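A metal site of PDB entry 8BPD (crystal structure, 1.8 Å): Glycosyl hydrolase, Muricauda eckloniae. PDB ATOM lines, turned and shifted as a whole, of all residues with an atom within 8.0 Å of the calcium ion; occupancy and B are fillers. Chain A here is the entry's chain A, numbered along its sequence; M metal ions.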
ATOM      1  N   ALA A  78     -28.042  -0.806  27.311  1.00  0.00           N
ATOM      2  CA  ALA A  78     -27.142  -1.207  26.234  1.00  0.00           C
ATOM      3  C   ALA A  78     -26.584  -2.622  26.413  1.00  0.00           C
ATOM      4  O   ALA A  78     -25.572  -2.959  25.810  1.00  0.00           O
ATOM      5  CB  ALA A  78     -25.989  -0.201  26.125  1.00  0.00           C
ATOM      6  N   TYR A  81     -27.977  -9.106  27.717  1.00  0.00           N
ATOM      7  CA  TYR A  81     -27.920 -10.322  28.500  1.00  0.00           C
ATOM      8  C   TYR A  81     -28.131 -10.089  29.978  1.00  0.00           C
ATOM      9  O   TYR A  81     -27.990 -11.024  30.754  1.00  0.00           O
ATOM     10  CB  TYR A  81     -26.604 -11.071  28.267  1.00  0.00           C
ATOM     11  CG  TYR A  81     -25.381 -10.214  28.115  1.00  0.00           C
ATOM     12  CD1 TYR A  81     -24.563 -10.315  26.995  1.00  0.00           C
ATOM     13  CD2 TYR A  81     -25.022  -9.296  29.104  1.00  0.00           C
ATOM     14  CE1 TYR A  81     -23.429  -9.500  26.831  1.00  0.00           C
ATOM     15  CE2 TYR A  81     -23.880  -8.500  28.969  1.00  0.00           C
ATOM     16  CZ  TYR A  81     -23.084  -8.599  27.826  1.00  0.00           C
ATOM     17  OH  TYR A  81     -21.964  -7.784  27.697  1.00  0.00           O
ATOM     18  N   ASP A 132     -30.492  -7.152  21.029  1.00  0.00           N
ATOM     19  CA  ASP A 132     -29.552  -8.102  20.463  1.00  0.00           C
ATOM     20  C   ASP A 132     -29.197  -9.197  21.441  1.00  0.00           C
ATOM     21  O   ASP A 132     -28.546 -10.180  21.058  1.00  0.00           O
ATOM     22  CB  ASP A 132     -28.290  -7.403  19.935  1.00  0.00           C
ATOM     23  CG  ASP A 132     -27.532  -6.628  20.980  1.00  0.00           C
ATOM     24  OD1 ASP A 132     -28.092  -6.242  22.006  1.00  0.00           O
ATOM     25  OD2 ASP A 132     -26.351  -6.358  20.719  1.00  0.00           O
ATOM     26  N   GLY A 133     -29.649  -9.092  22.682  1.00  0.00           N
ATOM     27  CA  GLY A 133     -29.671 -10.223  23.586  1.00  0.00           C
ATOM     28  C   GLY A 133     -28.279 -10.736  23.891  1.00  0.00           C
ATOM     29  O   GLY A 133     -27.296 -10.036  23.712  1.00  0.00           O
ATOM     30  N   PRO A 134     -28.187 -11.994  24.357  1.00  0.00           N
ATOM     31  CA  PRO A 134     -26.882 -12.537  24.775  1.00  0.00           C
ATOM     32  C   PRO A 134     -25.888 -12.751  23.636  1.00  0.00           C
ATOM     33  O   PRO A 134     -24.672 -12.804  23.906  1.00  0.00           O
ATOM     34  CB  PRO A 134     -27.254 -13.868  25.438  1.00  0.00           C
ATOM     35  CG  PRO A 134     -28.710 -13.680  25.882  1.00  0.00           C
ATOM     36  CD  PRO A 134     -29.309 -12.848  24.800  1.00  0.00           C
ATOM     37  N   SER A 135     -26.347 -12.894  22.390  1.00  0.00           N
ATOM     38  CA  SER A 135     -25.377 -13.039  21.290  1.00  0.00           C
ATOM     39  C   SER A 135     -24.681 -11.727  20.965  1.00  0.00           C
ATOM     40  O   SER A 135     -23.633 -11.728  20.307  1.00  0.00           O
ATOM     41  CB  SER A 135     -26.068 -13.596  20.061  1.00  0.00           C
ATOM     42  OG  SER A 135     -26.439 -14.958  20.314  1.00  0.00           O
ATOM     43  N   ALA A 136     -25.259 -10.610  21.404  1.00  0.00           N
ATOM     44  CA  ALA A 136     -24.630  -9.303  21.376  1.00  0.00           C
ATOM     45  C   ALA A 136     -24.096  -8.901  20.003  1.00  0.00           C
ATOM     46  O   ALA A 136     -23.034  -8.310  19.883  1.00  0.00           O
ATOM     47  CB  ALA A 136     -23.486  -9.248  22.407  1.00  0.00           C
ATOM     48  N   ARG A 137     -24.876  -9.142  18.944  1.00  0.00           N
ATOM     49  CA  ARG A 137     -24.356  -8.866  17.599  1.00  0.00           C
ATOM     50  C   ARG A 137     -24.520  -7.417  17.169  1.00  0.00           C
ATOM     51  O   ARG A 137     -24.102  -7.061  16.061  1.00  0.00           O
ATOM     52  CB  ARG A 137     -25.005  -9.798  16.579  1.00  0.00           C
ATOM     53  CG  ARG A 137     -24.675 -11.268  16.814  1.00  0.00           C
ATOM     54  CD  ARG A 137     -25.203 -12.156  15.697  1.00  0.00           C
ATOM     55  NE  ARG A 137     -24.726 -13.523  15.854  1.00  0.00           N
ATOM     56  CZ  ARG A 137     -25.425 -14.503  16.421  1.00  0.00           C
ATOM     57  NH1 ARG A 137     -26.683 -14.348  16.779  1.00  0.00           N
ATOM     58  NH2 ARG A 137     -24.823 -15.669  16.625  1.00  0.00           N
ATOM     59  N   SER A 138     -25.111  -6.582  18.017  1.00  0.00           N
ATOM     60  CA  SER A 138     -25.162  -5.148  17.798  1.00  0.00           C
ATOM     61  C   SER A 138     -24.445  -4.456  18.969  1.00  0.00           C
ATOM     62  O   SER A 138     -23.326  -4.877  19.302  1.00  0.00           O
ATOM     63  CB  SER A 138     -26.617  -4.691  17.630  1.00  0.00           C
ATOM     64  OG  SER A 138     -26.707  -3.309  17.414  1.00  0.00           O
ATOM     65  N   GLY A 139     -25.038  -3.457  19.604  1.00  0.00           N
ATOM     66  CA  GLY A 139     -24.323  -2.609  20.555  1.00  0.00           C
ATOM     67  C   GLY A 139     -24.008  -3.251  21.916  1.00  0.00           C
ATOM     68  O   GLY A 139     -23.212  -2.693  22.674  1.00  0.00           O
ATOM     69  N   THR A 140     -24.585  -4.409  22.249  1.00  0.00           N
ATOM     70  CA  THR A 140     -24.211  -5.022  23.515  1.00  0.00           C
ATOM     71  C   THR A 140     -22.724  -5.402  23.511  1.00  0.00           C
ATOM     72  O   THR A 140     -22.234  -6.009  22.564  1.00  0.00           O
ATOM     73  CB  THR A 140     -25.084  -6.239  23.813  1.00  0.00           C
ATOM     74  OG1 THR A 140     -26.448  -5.810  23.985  1.00  0.00           O
ATOM     75  CG2 THR A 140     -24.631  -6.986  25.104  1.00  0.00           C
ATOM     76  N   ARG A 141     -22.008  -5.034  24.555  1.00  0.00           N
ATOM     77  CA  ARG A 141     -20.594  -5.417  24.664  1.00  0.00           C
ATOM     78  C   ARG A 141     -20.423  -6.929  24.553  1.00  0.00           C
ATOM     79  O   ARG A 141     -21.138  -7.708  25.194  1.00  0.00           O
ATOM     80  CB  ARG A 141     -20.046  -4.909  25.997  1.00  0.00           C
ATOM     81  CG  ARG A 141     -18.544  -5.074  26.141  1.00  0.00           C
ATOM     82  CD  ARG A 141     -18.020  -4.825  27.595  1.00  0.00           C
ATOM     83  NE  ARG A 141     -16.554  -4.905  27.644  1.00  0.00           N
ATOM     84  CZ  ARG A 141     -15.827  -5.079  28.749  1.00  0.00           C
ATOM     85  NH1 ARG A 141     -16.390  -5.190  29.950  1.00  0.00           N
ATOM     86  NH2 ARG A 141     -14.495  -5.138  28.652  1.00  0.00           N
ATOM     87  N   ASN A 142     -19.478  -7.356  23.718  1.00  0.00           N
ATOM     88  CA  ASN A 142     -19.300  -8.781  23.529  1.00  0.00           C
ATOM     89  C   ASN A 142     -18.775  -9.439  24.797  1.00  0.00           C
ATOM     90  O   ASN A 142     -17.881  -8.919  25.472  1.00  0.00           O
ATOM     91  CB  ASN A 142     -18.346  -9.064  22.365  1.00  0.00           C
ATOM     92  CG  ASN A 142     -18.911  -8.627  21.031  1.00  0.00           C
ATOM     93  OD1 ASN A 142     -20.005  -8.102  20.959  1.00  0.00           O
ATOM     94  ND2 ASN A 142     -18.147  -8.847  19.980  1.00  0.00           N
ATOM     95  N   ASN A 143     -19.360 -10.593  25.124  1.00  0.00           N
ATOM     96  CA  ASN A 143     -18.966 -11.390  26.269  1.00  0.00           C
ATOM     97  C   ASN A 143     -18.993 -12.843  25.821  1.00  0.00           C
ATOM     98  O   ASN A 143     -20.060 -13.435  25.594  1.00  0.00           O
ATOM     99  CB  ASN A 143     -19.903 -11.146  27.457  1.00  0.00           C
ATOM    100  CG  ASN A 143     -19.452 -11.895  28.696  1.00  0.00           C
ATOM    101  OD1 ASN A 143     -19.190 -13.094  28.623  1.00  0.00           O
ATOM    102  ND2 ASN A 143     -19.325 -11.202  29.817  1.00  0.00           N
ATOM    103  N   HIS A 188     -30.815  -1.734  19.606  1.00  0.00           N
ATOM    104  CA  HIS A 188     -29.880  -2.721  19.041  1.00  0.00           C
ATOM    105  C   HIS A 188     -30.577  -3.658  18.063  1.00  0.00           C
ATOM    106  O   HIS A 188     -30.199  -4.824  17.927  1.00  0.00           O
ATOM    107  CB  HIS A 188     -29.210  -3.548  20.138  1.00  0.00           C
ATOM    108  CG  HIS A 188     -28.357  -2.763  21.081  1.00  0.00           C
ATOM    109  ND1 HIS A 188     -27.742  -3.349  22.171  1.00  0.00           N
ATOM    110  CD2 HIS A 188     -27.967  -1.469  21.079  1.00  0.00           C
ATOM    111  CE1 HIS A 188     -27.019  -2.443  22.813  1.00  0.00           C
ATOM    112  NE2 HIS A 188     -27.132  -1.294  22.167  1.00  0.00           N
HETATM  113 CA    CA M   1     -21.712  -6.467  20.258  1.00  0.00          CA
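The backbone carbonyl oxygen of Ala 78 lies close to the side-chain hydroxyl of Thr 140.
The side-chain hydroxyl (OG1) of Thr 140 is in hydrogen-bond range of a ring nitrogen (ND1) of His 188, 3.3 Å away.
The side-chain carboxylate (OD2) of Asp 132 sits at hydrogen-bond distance from the backbone NH (N) of Ser 138 (3.0 Å).
OG1 of Thr 140 lies within hydrogen-bond range of OD1 of Asp 132 (2.6 Å).
The calcium ion is bound by the backbone carbonyl oxygen of Ala 136 (2.3 Å), the backbone carbonyl oxygen of Thr 140 (2.4 Å), the backbone carbonyl oxygen of Ser 138 (2.5 Å) and the side-chain amide oxygen of Asn 142 (2.5 Å).
Within 4 Å of the calcium ion: Ala 136, Ser 138, Thr 140 and Asn 142.
Along chain A the residues within 4 Å of the calcium ion span positions 136 to 142.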
